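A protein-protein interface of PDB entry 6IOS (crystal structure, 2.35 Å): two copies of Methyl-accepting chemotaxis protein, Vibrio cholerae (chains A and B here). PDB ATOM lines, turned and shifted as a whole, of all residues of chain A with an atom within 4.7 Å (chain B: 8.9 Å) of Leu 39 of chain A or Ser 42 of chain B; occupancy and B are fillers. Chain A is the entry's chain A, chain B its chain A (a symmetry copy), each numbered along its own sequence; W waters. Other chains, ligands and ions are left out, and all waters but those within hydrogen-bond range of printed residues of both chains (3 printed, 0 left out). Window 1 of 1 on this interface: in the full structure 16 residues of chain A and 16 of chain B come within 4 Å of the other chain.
The side-chain hydroxyl (OG) of Ser 35 of chain B sits at hydrogen-bond distance from the side-chain hydroxyl (OG) of Ser 35 of chain A, 3.0 Å away. O of Gly 38 of chain A sits close to OD1 of Asn 65 of chain B, 3.3 Å away. OG of Ser 42 of chain A sits at hydrogen-bond distance from OD1 of Asn 65 of chain B (2.9 Å). N of Leu 66 of chain B sits at hydrogen-bond distance from OG of Ser 42 of chain A, 3.4 Å away. The side-chain amide oxygen (OD1) of Asn 65 of chain A lies close to the backbone carbonyl oxygen (O) of Gly 38 of chain B, at 3.3 Å. OD1 of Asn 65 of chain A lies within hydrogen-bond range of OG of Ser 42 of chain B, 2.9 Å away. The side-chain carboxylate (OE1) of Glu 45 of chain B is in hydrogen-bond range of the backbone NH (N) of Asn 65 of chain A (2.8 Å). The backbone NH of Leu 66 of chain A is in hydrogen-bond range of the side-chain hydroxyl of Ser 42 of chain B (3.4 Å).
The backbone carbonyl oxygen (O) of Leu 39 of chain A lies within hydrogen-bond range of the side-chain hydroxyl (OG1) of Thr 43 of chain A (2.6 Å). The backbone carbonyl oxygen of Asn 65 of chain A lies within hydrogen-bond range of the side-chain hydroxyl of Ser 69 of chain A, 2.7 Å away. O of Leu 39 of chain B sits at hydrogen-bond distance from OG1 of Thr 43 of chain B (2.6 Å). The side-chain amide nitrogen of Gln 41 of chain B is in hydrogen-bond range of the side-chain carboxylate of Glu 45 of chain B, 3.1 Å away. The side-chain hydroxyl (OG) of Ser 69 of chain B sits at hydrogen-bond distance from the backbone carbonyl oxygen (O) of Asn 65 of chain B, at 2.7 Å.
Among the printed residues, merely in contact across the chains: Leu 39 of chain A with Ser 42 of chain B (3.8 Å), Gln 41 of chain A with Asn 65 of chain B (3.7 Å), Ser 42 of chain A with Leu 39 of chain B (3.8 Å) and Asn 65 of chain A with Gln 41 of chain B (3.7 Å).
Of chain B, only Ser 42 (3.8 Å) comes within 4 Å of Leu 39 of chain A. Ser 42 of chain B touches just these residues of chain A: Leu 39 (3.8 Å), Asn 65 (2.9 Å) and Leu 66 (3.4 Å). Gly 38 of chain A touches just one residue of chain B: Asn 65 (3.3 Å). Of the printed residues of chain A, Glu 45 of chain B touches Asn 65. Of the printed residues of chain A, Leu 39 of chain B touches Ser 42 (3.8 Å). Of the printed residues of chain A, Leu 66 of chain B touches Ser 42. Printed residues of chain A within 4 Å of Gly 38 of chain B: Asn 65. Thr 44 of chain B touches none of the printed residues of chain A. Tyr 147 of chain B touches none of the printed residues of chain A.
Of the 13 printed residues of chain A, 7 touch a printed residue of chain B. Hydrophobic or aromatic side chains of chain A that line the printed part of chain B: Leu 39 and Leu 66. Hydrophobic or aromatic side chains of chain B within 4 Å of the printed part of chain A: Leu 39 and Leu 66.
Ser 35 of chain B touches its own counterpart, Ser 35 of chain A. Leu 39 of chain A touches Ser 42 of chain B, and with the chains exchanged Ser 42 of chain A touches Leu 39 of chain B. Gln 41 of chain A touches Asn 65 of chain B, and with the chains exchanged Asn 65 of chain A touches Gln 41 of chain B. Ser 42 of chain A touches Leu 66 of chain B, and with the chains exchanged Leu 66 of chain A touches Ser 42 of chain B. 12 positions are printed for both chains. Of the 12 pairs that touch across the chains among the printed residues, 11 have their exchanged pair printed and touching as well.
Water W1 lies within hydrogen-bond range of OE1 of Glu 45 of chain B (2.6 Å), N of Leu 66 of chain A (2.9 Å), OG of Ser 42 of chain B (3.1 Å) and N of Asn 65 of chain A (3.5 Å). Water W2 lies within hydrogen-bond range of the backbone NH (N) of Leu 66 of chain B (2.9 Å), the side-chain hydroxyl (OG) of Ser 42 of chain A (3.1 Å) and the backbone NH (N) of Asn 65 of chain B (3.5 Å). Water W3 bridges O of Ser 35 of chain B (3.1 Å) and O of Ser 35 of chain A (3.1 Å).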
ATOM      1  N   SER A  35      23.792  25.868 -31.211  1.00  0.00           N
ATOM      2  CA  SER A  35      23.786  26.597 -29.954  1.00  0.00           C
ATOM      3  C   SER A  35      22.374  27.031 -29.549  1.00  0.00           C
ATOM      4  O   SER A  35      21.981  26.872 -28.396  1.00  0.00           O
ATOM      5  CB  SER A  35      24.691  27.815 -30.063  1.00  0.00           C
ATOM      6  OG  SER A  35      24.672  28.540 -28.856  1.00  0.00           O
ATOM      7  N   LYS A  36      21.623  27.600 -30.484  1.00  0.00           N
ATOM      8  CA  LYS A  36      20.233  27.963 -30.213  1.00  0.00           C
ATOM      9  C   LYS A  36      19.405  26.721 -29.890  1.00  0.00           C
ATOM     10  O   LYS A  36      18.564  26.746 -28.993  1.00  0.00           O
ATOM     11  CB  LYS A  36      19.608  28.695 -31.401  1.00  0.00           C
ATOM     12  CG  LYS A  36      19.949  30.172 -31.526  1.00  0.00           C
ATOM     13  CD  LYS A  36      19.566  30.651 -32.943  1.00  0.00           C
ATOM     14  CE  LYS A  36      19.725  32.162 -33.152  1.00  0.00           C
ATOM     15  NZ  LYS A  36      21.033  32.665 -32.656  1.00  0.00           N
ATOM     16  N   LYS A  37      19.653  25.627 -30.607  1.00  0.00           N
ATOM     17  CA  LYS A  37      18.943  24.382 -30.324  1.00  0.00           C
ATOM     18  C   LYS A  37      19.263  23.839 -28.938  1.00  0.00           C
ATOM     19  O   LYS A  37      18.386  23.305 -28.274  1.00  0.00           O
ATOM     20  CB  LYS A  37      19.257  23.319 -31.362  1.00  0.00           C
ATOM     21  CG  LYS A  37      18.655  23.583 -32.731  1.00  0.00           C
ATOM     22  CD  LYS A  37      19.131  22.540 -33.723  1.00  0.00           C
ATOM     23  CE  LYS A  37      18.458  22.719 -35.074  1.00  0.00           C
ATOM     24  NZ  LYS A  37      18.925  21.694 -36.049  1.00  0.00           N
ATOM     25  N   GLY A  38      20.509  23.973 -28.500  1.00  0.00           N
ATOM     26  CA  GLY A  38      20.875  23.554 -27.159  1.00  0.00           C
ATOM     27  C   GLY A  38      20.128  24.369 -26.116  1.00  0.00           C
ATOM     28  O   GLY A  38      19.590  23.824 -25.152  1.00  0.00           O
ATOM     29  N   LEU A  39      20.076  25.677 -26.326  1.00  0.00           N
ATOM     30  CA  LEU A  39      19.422  26.584 -25.389  1.00  0.00           C
ATOM     31  C   LEU A  39      17.923  26.313 -25.326  1.00  0.00           C
ATOM     32  O   LEU A  39      17.312  26.354 -24.254  1.00  0.00           O
ATOM     33  CB  LEU A  39      19.700  28.032 -25.797  1.00  0.00           C
ATOM     34  CG  LEU A  39      19.397  29.153 -24.798  1.00  0.00           C
ATOM     35  CD1 LEU A  39      19.920  28.802 -23.397  1.00  0.00           C
ATOM     36  CD2 LEU A  39      19.976  30.488 -25.274  1.00  0.00           C
ATOM     37  N   ALA A  40      17.333  26.014 -26.479  1.00  0.00           N
ATOM     38  CA  ALA A  40      15.916  25.683 -26.566  1.00  0.00           C
ATOM     39  C   ALA A  40      15.582  24.327 -25.946  1.00  0.00           C
ATOM     40  O   ALA A  40      14.556  24.190 -25.281  1.00  0.00           O
ATOM     41  CB  ALA A  40      15.457  25.710 -28.023  1.00  0.00           C
ATOM     42  N   GLN A  41      16.430  23.327 -26.182  1.00  0.00           N
ATOM     43  CA  GLN A  41      16.211  21.998 -25.626  1.00  0.00           C
ATOM     44  C   GLN A  41      16.259  22.027 -24.089  1.00  0.00           C
ATOM     45  O   GLN A  41      15.390  21.464 -23.417  1.00  0.00           O
ATOM     46  CB  GLN A  41      17.249  21.009 -26.165  1.00  0.00           C
ATOM     47  CG  GLN A  41      17.035  19.579 -25.681  1.00  0.00           C
ATOM     48  CD  GLN A  41      15.794  18.947 -26.294  1.00  0.00           C
ATOM     49  OE1 GLN A  41      15.431  19.269 -27.425  1.00  0.00           O
ATOM     50  NE2 GLN A  41      15.129  18.056 -25.548  1.00  0.00           N
ATOM     51  N   SER A  42      17.277  22.699 -23.550  1.00  0.00           N
ATOM     52  CA  SER A  42      17.461  22.806 -22.115  1.00  0.00           C
ATOM     53  C   SER A  42      16.351  23.611 -21.459  1.00  0.00           C
ATOM     54  O   SER A  42      15.896  23.267 -20.368  1.00  0.00           O
ATOM     55  CB  SER A  42      18.821  23.429 -21.784  1.00  0.00           C
ATOM     56  OG  SER A  42      19.856  22.474 -21.914  1.00  0.00           O
ATOM     57  N   THR A  43      15.914  24.679 -22.115  1.00  0.00           N
ATOM     58  CA  THR A  43      14.823  25.489 -21.562  1.00  0.00           C
ATOM     59  C   THR A  43      13.552  24.650 -21.504  1.00  0.00           C
ATOM     60  O   THR A  43      12.821  24.696 -20.526  1.00  0.00           O
ATOM     61  CB  THR A  43      14.566  26.774 -22.384  1.00  0.00           C
ATOM     62  OG1 THR A  43      15.780  27.546 -22.469  1.00  0.00           O
ATOM     63  CG2 THR A  43      13.471  27.619 -21.745  1.00  0.00           C
ATOM     64  N   ASN A  65      19.547  36.492 -20.228  1.00  0.00           N
ATOM     65  CA  ASN A  65      20.343  35.880 -21.266  1.00  0.00           C
ATOM     66  C   ASN A  65      19.463  35.104 -22.248  1.00  0.00           C
ATOM     67  O   ASN A  65      19.615  35.235 -23.461  1.00  0.00           O
ATOM     68  CB  ASN A  65      21.412  34.969 -20.671  1.00  0.00           C
ATOM     69  CG  ASN A  65      22.334  34.400 -21.742  1.00  0.00           C
ATOM     70  OD1 ASN A  65      22.137  33.282 -22.236  1.00  0.00           O
ATOM     71  ND2 ASN A  65      23.320  35.186 -22.136  1.00  0.00           N
ATOM     72  N   LEU A  66      18.529  34.320 -21.723  1.00  0.00           N
ATOM     73  CA  LEU A  66      17.631  33.538 -22.570  1.00  0.00           C
ATOM     74  C   LEU A  66      16.768  34.456 -23.414  1.00  0.00           C
ATOM     75  O   LEU A  66      16.714  34.333 -24.631  1.00  0.00           O
ATOM     76  CB  LEU A  66      16.766  32.612 -21.711  1.00  0.00           C
ATOM     77  CG  LEU A  66      15.701  31.764 -22.405  1.00  0.00           C
ATOM     78  CD1 LEU A  66      16.290  30.817 -23.478  1.00  0.00           C
ATOM     79  CD2 LEU A  66      14.901  30.991 -21.362  1.00  0.00           C
ATOM     80  N   SER A  69      18.403  35.974 -26.370  1.00  0.00           N
ATOM     81  CA  SER A  69      18.989  35.073 -27.385  1.00  0.00           C
ATOM     82  C   SER A  69      18.031  34.758 -28.529  1.00  0.00           C
ATOM     83  O   SER A  69      18.411  34.131 -29.501  1.00  0.00           O
ATOM     84  CB  SER A  69      19.448  33.756 -26.751  1.00  0.00           C
ATOM     85  OG  SER A  69      20.365  33.984 -25.696  1.00  0.00           O
ATOM     86  N   PHE A  70      16.778  35.183 -28.387  1.00  0.00           N
ATOM     87  CA  PHE A  70      15.741  34.904 -29.365  1.00  0.00           C
ATOM     88  C   PHE A  70      14.881  36.146 -29.535  1.00  0.00           C
ATOM     89  O   PHE A  70      14.796  36.982 -28.642  1.00  0.00           O
ATOM     90  CB  PHE A  70      14.877  33.708 -28.935  1.00  0.00           C
ATOM     91  CG  PHE A  70      15.619  32.395 -28.926  1.00  0.00           C
ATOM     92  CD1 PHE A  70      15.851  31.708 -30.112  1.00  0.00           C
ATOM     93  CD2 PHE A  70      16.088  31.855 -27.737  1.00  0.00           C
ATOM     94  CE1 PHE A  70      16.535  30.507 -30.118  1.00  0.00           C
ATOM     95  CE2 PHE A  70      16.775  30.655 -27.737  1.00  0.00           C
ATOM     96  CZ  PHE A  70      16.993  29.977 -28.932  1.00  0.00           C
ATOM     97  N   ALA B  34      31.347  30.275 -26.750  1.00  0.00           N
ATOM     98  CA  ALA B  34      30.251  31.224 -26.603  1.00  0.00           C
ATOM     99  C   ALA B  34      28.944  30.493 -26.304  1.00  0.00           C
ATOM    100  O   ALA B  34      28.123  30.943 -25.505  1.00  0.00           O
ATOM    101  CB  ALA B  34      30.113  32.061 -27.852  1.00  0.00           C
ATOM    102  N   SER B  35      28.770  29.350 -26.951  1.00  0.00           N
ATOM    103  CA  SER B  35      27.604  28.509 -26.746  1.00  0.00           C
ATOM    104  C   SER B  35      27.551  27.937 -25.326  1.00  0.00           C
ATOM    105  O   SER B  35      26.505  27.959 -24.684  1.00  0.00           O
ATOM    106  CB  SER B  35      27.601  27.377 -27.761  1.00  0.00           C
ATOM    107  OG  SER B  35      26.485  26.544 -27.554  1.00  0.00           O
ATOM    108  N   LYS B  36      28.668  27.402 -24.847  1.00  0.00           N
ATOM    109  CA  LYS B  36      28.736  26.913 -23.471  1.00  0.00           C
ATOM    110  C   LYS B  36      28.512  28.056 -22.482  1.00  0.00           C
ATOM    111  O   LYS B  36      27.826  27.886 -21.476  1.00  0.00           O
ATOM    112  CB  LYS B  36      30.084  26.250 -23.183  1.00  0.00           C
ATOM    113  CG  LYS B  36      30.240  24.821 -23.678  1.00  0.00           C
ATOM    114  CD  LYS B  36      31.738  24.448 -23.651  1.00  0.00           C
ATOM    115  CE  LYS B  36      32.019  22.978 -23.990  1.00  0.00           C
ATOM    116  NZ  LYS B  36      31.286  22.530 -25.203  1.00  0.00           N
ATOM    117  N   LYS B  37      29.074  29.226 -22.774  1.00  0.00           N
ATOM    118  CA  LYS B  37      28.862  30.384 -21.908  1.00  0.00           C
ATOM    119  C   LYS B  37      27.404  30.819 -21.875  1.00  0.00           C
ATOM    120  O   LYS B  37      26.910  31.223 -20.831  1.00  0.00           O
ATOM    121  CB  LYS B  37      29.725  31.558 -22.337  1.00  0.00           C
ATOM    122  CG  LYS B  37      31.207  31.378 -22.066  1.00  0.00           C
ATOM    123  CD  LYS B  37      31.991  32.541 -22.643  1.00  0.00           C
ATOM    124  CE  LYS B  37      33.466  32.438 -22.293  1.00  0.00           C
ATOM    125  NZ  LYS B  37      34.236  33.581 -22.859  1.00  0.00           N
ATOM    126  N   GLY B  38      26.713  30.738 -23.007  1.00  0.00           N
ATOM    127  CA  GLY B  38      25.298  31.057 -23.038  1.00  0.00           C
ATOM    128  C   GLY B  38      24.507  30.096 -22.166  1.00  0.00           C
ATOM    129  O   GLY B  38      23.648  30.508 -21.387  1.00  0.00           O
ATOM    130  N   LEU B  39      24.820  28.813 -22.281  1.00  0.00           N
ATOM    131  CA  LEU B  39      24.120  27.776 -21.529  1.00  0.00           C
ATOM    132  C   LEU B  39      24.367  27.929 -20.033  1.00  0.00           C
ATOM    133  O   LEU B  39      23.462  27.744 -19.214  1.00  0.00           O
ATOM    134  CB  LEU B  39      24.563  26.397 -22.020  1.00  0.00           C
ATOM    135  CG  LEU B  39      23.741  25.170 -21.616  1.00  0.00           C
ATOM    136  CD1 LEU B  39      22.237  25.428 -21.795  1.00  0.00           C
ATOM    137  CD2 LEU B  39      24.176  23.931 -22.404  1.00  0.00           C
ATOM    138  N   ALA B  40      25.596  28.289 -19.676  1.00  0.00           N
ATOM    139  CA  ALA B  40      25.967  28.520 -18.285  1.00  0.00           C
ATOM    140  C   ALA B  40      25.338  29.785 -17.704  1.00  0.00           C
ATOM    141  O   ALA B  40      24.906  29.783 -16.552  1.00  0.00           O
ATOM    142  CB  ALA B  40      27.488  28.594 -18.151  1.00  0.00           C
ATOM    143  N   GLN B  41      25.307  30.863 -18.486  1.00  0.00           N
ATOM    144  CA  GLN B  41      24.715  32.114 -18.032  1.00  0.00           C
ATOM    145  C   GLN B  41      23.211  31.947 -17.755  1.00  0.00           C
ATOM    146  O   GLN B  41      22.707  32.380 -16.715  1.00  0.00           O
ATOM    147  CB  GLN B  41      24.939  33.224 -19.065  1.00  0.00           C
ATOM    148  CG  GLN B  41      24.409  34.582 -18.622  1.00  0.00           C
ATOM    149  CD  GLN B  41      25.230  35.175 -17.487  1.00  0.00           C
ATOM    150  OE1 GLN B  41      26.434  34.933 -17.404  1.00  0.00           O
ATOM    151  NE2 GLN B  41      24.585  35.941 -16.599  1.00  0.00           N
ATOM    152  N   SER B  42      22.513  31.305 -18.693  1.00  0.00           N
ATOM    153  CA  SER B  42      21.085  31.080 -18.577  1.00  0.00           C
ATOM    154  C   SER B  42      20.751  30.138 -17.432  1.00  0.00           C
ATOM    155  O   SER B  42      19.764  30.345 -16.726  1.00  0.00           O
ATOM    156  CB  SER B  42      20.511  30.532 -19.887  1.00  0.00           C
ATOM    157  OG  SER B  42      20.339  31.569 -20.833  1.00  0.00           O
ATOM    158  N   THR B  43      21.564  29.106 -17.245  1.00  0.00           N
ATOM    159  CA  THR B  43      21.326  28.170 -16.141  1.00  0.00           C
ATOM    160  C   THR B  43      21.486  28.903 -14.814  1.00  0.00           C
ATOM    161  O   THR B  43      20.698  28.713 -13.899  1.00  0.00           O
ATOM    162  CB  THR B  43      22.277  26.950 -16.185  1.00  0.00           C
ATOM    163  OG1 THR B  43      22.150  26.281 -17.455  1.00  0.00           O
ATOM    164  CG2 THR B  43      21.958  25.971 -15.061  1.00  0.00           C
ATOM    165  N   THR B  44      22.499  29.760 -14.722  1.00  0.00           N
ATOM    166  CA  THR B  44      22.739  30.497 -13.490  1.00  0.00           C
ATOM    167  C   THR B  44      21.571  31.439 -13.199  1.00  0.00           C
ATOM    168  O   THR B  44      21.061  31.474 -12.073  1.00  0.00           O
ATOM    169  CB  THR B  44      24.066  31.282 -13.558  1.00  0.00           C
ATOM    170  OG1 THR B  44      25.146  30.364 -13.784  1.00  0.00           O
ATOM    171  CG2 THR B  44      24.313  32.053 -12.252  1.00  0.00           C
ATOM    172  N   GLU B  45      21.127  32.172 -14.220  1.00  0.00           N
ATOM    173  CA  GLU B  45      20.011  33.105 -14.082  1.00  0.00           C
ATOM    174  C   GLU B  45      18.725  32.393 -13.653  1.00  0.00           C
ATOM    175  O   GLU B  45      17.947  32.913 -12.848  1.00  0.00           O
ATOM    176  CB  GLU B  45      19.793  33.864 -15.387  1.00  0.00           C
ATOM    177  CG  GLU B  45      20.876  34.895 -15.626  1.00  0.00           C
ATOM    178  CD  GLU B  45      20.775  35.606 -16.953  1.00  0.00           C
ATOM    179  OE1 GLU B  45      19.902  35.255 -17.779  1.00  0.00           O
ATOM    180  OE2 GLU B  45      21.593  36.527 -17.180  1.00  0.00           O
ATOM    181  N   ILE B  46      18.504  31.199 -14.190  1.00  0.00           N
ATOM    182  CA  ILE B  46      17.322  30.428 -13.838  1.00  0.00           C
ATOM    183  C   ILE B  46      17.432  29.934 -12.403  1.00  0.00           C
ATOM    184  O   ILE B  46      16.444  29.919 -11.668  1.00  0.00           O
ATOM    185  CB  ILE B  46      17.104  29.256 -14.803  1.00  0.00           C
ATOM    186  CG1 ILE B  46      16.711  29.800 -16.190  1.00  0.00           C
ATOM    187  CG2 ILE B  46      16.024  28.331 -14.274  1.00  0.00           C
ATOM    188  CD1 ILE B  46      16.782  28.793 -17.320  1.00  0.00           C
ATOM    189  N   LEU B  47      18.633  29.577 -11.971  1.00  0.00           N
ATOM    190  CA  LEU B  47      18.793  29.173 -10.579  1.00  0.00           C
ATOM    191  C   LEU B  47      18.570  30.372  -9.668  1.00  0.00           C
ATOM    192  O   LEU B  47      18.051  30.213  -8.563  1.00  0.00           O
ATOM    193  CB  LEU B  47      20.169  28.537 -10.338  1.00  0.00           C
ATOM    194  CG  LEU B  47      20.286  27.136 -10.958  1.00  0.00           C
ATOM    195  CD1 LEU B  47      21.395  26.334 -10.328  1.00  0.00           C
ATOM    196  CD2 LEU B  47      18.965  26.379 -10.879  1.00  0.00           C
ATOM    197  N   GLN B  48      18.925  31.575 -10.138  1.00  0.00           N
ATOM    198  CA  GLN B  48      18.704  32.805  -9.354  1.00  0.00           C
ATOM    199  C   GLN B  48      17.219  33.184  -9.161  1.00  0.00           C
ATOM    200  O   GLN B  48      16.904  34.073  -8.381  1.00  0.00           O
ATOM    201  CB  GLN B  48      19.469  33.983  -9.976  1.00  0.00           C
ATOM    202  CG  GLN B  48      20.902  34.064  -9.495  1.00  0.00           C
ATOM    203  CD  GLN B  48      21.736  35.148 -10.181  1.00  0.00           C
ATOM    204  OE1 GLN B  48      22.901  35.334  -9.846  1.00  0.00           O
ATOM    205  NE2 GLN B  48      21.146  35.859 -11.136  1.00  0.00           N
ATOM    206  N   LEU B  49      16.301  32.490  -9.824  1.00  0.00           N
ATOM    207  CA  LEU B  49      14.877  32.677  -9.525  1.00  0.00           C
ATOM    208  C   LEU B  49      14.550  32.178  -8.115  1.00  0.00           C
ATOM    209  O   LEU B  49      13.562  32.603  -7.501  1.00  0.00           O
ATOM    210  CB  LEU B  49      13.998  31.952 -10.543  1.00  0.00           C
ATOM    211  CG  LEU B  49      14.168  32.362 -12.006  1.00  0.00           C
ATOM    212  CD1 LEU B  49      13.375  31.431 -12.892  1.00  0.00           C
ATOM    213  CD2 LEU B  49      13.739  33.813 -12.197  1.00  0.00           C
ATOM    214  N   PHE B  56      15.481  22.572  -6.117  1.00  0.00           N
ATOM    215  CA  PHE B  56      15.247  23.138  -7.440  1.00  0.00           C
ATOM    216  C   PHE B  56      16.525  23.036  -8.270  1.00  0.00           C
ATOM    217  O   PHE B  56      16.502  22.577  -9.405  1.00  0.00           O
ATOM    218  CB  PHE B  56      14.776  24.597  -7.339  1.00  0.00           C
ATOM    219  CG  PHE B  56      14.685  25.297  -8.670  1.00  0.00           C
ATOM    220  CD1 PHE B  56      13.948  24.748  -9.711  1.00  0.00           C
ATOM    221  CD2 PHE B  56      15.337  26.498  -8.882  1.00  0.00           C
ATOM    222  CE1 PHE B  56      13.869  25.393 -10.943  1.00  0.00           C
ATOM    223  CE2 PHE B  56      15.252  27.157 -10.118  1.00  0.00           C
ATOM    224  CZ  PHE B  56      14.526  26.599 -11.143  1.00  0.00           C
ATOM    225  N   VAL B  60      17.272  20.855 -11.922  1.00  0.00           N
ATOM    226  CA  VAL B  60      17.715  21.537 -13.123  1.00  0.00           C
ATOM    227  C   VAL B  60      19.009  20.912 -13.630  1.00  0.00           C
ATOM    228  O   VAL B  60      19.146  20.651 -14.835  1.00  0.00           O
ATOM    229  CB  VAL B  60      17.891  23.063 -12.873  1.00  0.00           C
ATOM    230  CG1 VAL B  60      18.684  23.719 -13.999  1.00  0.00           C
ATOM    231  CG2 VAL B  60      16.532  23.741 -12.693  1.00  0.00           C
ATOM    232  N   ASN B  65      19.806  17.471 -21.469  1.00  0.00           N
ATOM    233  CA  ASN B  65      20.596  18.233 -22.408  1.00  0.00           C
ATOM    234  C   ASN B  65      21.687  19.029 -21.689  1.00  0.00           C
ATOM    235  O   ASN B  65      22.844  19.023 -22.107  1.00  0.00           O
ATOM    236  CB  ASN B  65      19.715  19.163 -23.238  1.00  0.00           C
ATOM    237  CG  ASN B  65      20.512  19.895 -24.309  1.00  0.00           C
ATOM    238  OD1 ASN B  65      20.953  21.036 -24.119  1.00  0.00           O
ATOM    239  ND2 ASN B  65      20.737  19.224 -25.425  1.00  0.00           N
ATOM    240  N   LEU B  66      21.324  19.691 -20.597  1.00  0.00           N
ATOM    241  CA  LEU B  66      22.287  20.479 -19.831  1.00  0.00           C
ATOM    242  C   LEU B  66      23.365  19.581 -19.255  1.00  0.00           C
ATOM    243  O   LEU B  66      24.552  19.812 -19.450  1.00  0.00           O
ATOM    244  CB  LEU B  66      21.572  21.255 -18.721  1.00  0.00           C
ATOM    245  CG  LEU B  66      22.418  22.082 -17.754  1.00  0.00           C
ATOM    246  CD1 LEU B  66      23.263  23.165 -18.468  1.00  0.00           C
ATOM    247  CD2 LEU B  66      21.522  22.693 -16.683  1.00  0.00           C
ATOM    248  N   SER B  69      25.994  18.468 -21.614  1.00  0.00           N
ATOM    249  CA  SER B  69      26.786  19.500 -22.317  1.00  0.00           C
ATOM    250  C   SER B  69      28.086  19.848 -21.599  1.00  0.00           C
ATOM    251  O   SER B  69      28.901  20.588 -22.117  1.00  0.00           O
ATOM    252  CB  SER B  69      25.970  20.784 -22.507  1.00  0.00           C
ATOM    253  OG  SER B  69      24.760  20.527 -23.196  1.00  0.00           O
ATOM    254  N   LEU B 113      30.743  35.832 -15.168  1.00  0.00           N
ATOM    255  CA  LEU B 113      31.181  34.582 -15.767  1.00  0.00           C
ATOM    256  C   LEU B 113      32.680  34.595 -16.037  1.00  0.00           C
ATOM    257  O   LEU B 113      33.197  35.555 -16.565  1.00  0.00           O
ATOM    258  CB  LEU B 113      30.419  34.321 -17.075  1.00  0.00           C
ATOM    259  CG  LEU B 113      30.653  32.948 -17.728  1.00  0.00           C
ATOM    260  CD1 LEU B 113      29.392  32.447 -18.440  1.00  0.00           C
ATOM    261  CD2 LEU B 113      31.832  32.958 -18.682  1.00  0.00           C
ATOM    262  N   THR B 133      30.468  30.833 -12.559  1.00  0.00           N
ATOM    263  CA  THR B 133      29.541  31.949 -12.474  1.00  0.00           C
ATOM    264  C   THR B 133      29.221  32.286 -11.027  1.00  0.00           C
ATOM    265  O   THR B 133      29.162  31.401 -10.175  1.00  0.00           O
ATOM    266  CB  THR B 133      28.192  31.666 -13.210  1.00  0.00           C
ATOM    267  OG1 THR B 133      27.571  30.484 -12.672  1.00  0.00           O
ATOM    268  CG2 THR B 133      28.402  31.515 -14.706  1.00  0.00           C
ATOM    269  N   MET B 145      28.897  28.805  -9.231  1.00  0.00           N
ATOM    270  CA  MET B 145      28.696  27.580  -9.981  1.00  0.00           C
ATOM    271  C   MET B 145      29.943  27.198 -10.749  1.00  0.00           C
ATOM    272  O   MET B 145      30.731  28.073 -11.122  1.00  0.00           O
ATOM    273  CB  MET B 145      27.533  27.729 -10.956  1.00  0.00           C
ATOM    274  CG  MET B 145      26.203  28.020 -10.291  1.00  0.00           C
ATOM    275  SD  MET B 145      24.834  27.745 -11.422  1.00  0.00           S
ATOM    276  CE  MET B 145      24.884  25.965 -11.558  1.00  0.00           C
ATOM    277  N   TYR B 147      30.944  24.802 -14.278  1.00  0.00           N
ATOM    278  CA  TYR B 147      30.595  23.961 -15.427  1.00  0.00           C
ATOM    279  C   TYR B 147      31.909  23.419 -15.985  1.00  0.00           C
ATOM    280  O   TYR B 147      32.644  24.139 -16.654  1.00  0.00           O
ATOM    281  CB  TYR B 147      29.822  24.736 -16.505  1.00  0.00           C
ATOM    282  CG  TYR B 147      28.581  25.441 -15.999  1.00  0.00           C
ATOM    283  CD1 TYR B 147      28.682  26.565 -15.163  1.00  0.00           C
ATOM    284  CD2 TYR B 147      27.312  24.986 -16.334  1.00  0.00           C
ATOM    285  CE1 TYR B 147      27.554  27.207 -14.672  1.00  0.00           C
ATOM    286  CE2 TYR B 147      26.164  25.640 -15.855  1.00  0.00           C
ATOM    287  CZ  TYR B 147      26.303  26.745 -15.031  1.00  0.00           C
ATOM    288  OH  TYR B 147      25.197  27.381 -14.546  1.00  0.00           O
HETATM  289  O   HOH W   1      18.627  33.373 -18.952  1.00  0.00           O
HETATM  290  O   HOH W   2      18.536  20.382 -20.015  1.00  0.00           O
HETATM  291  O   HOH W   3      23.767  27.370 -25.947  1.00  0.00           O
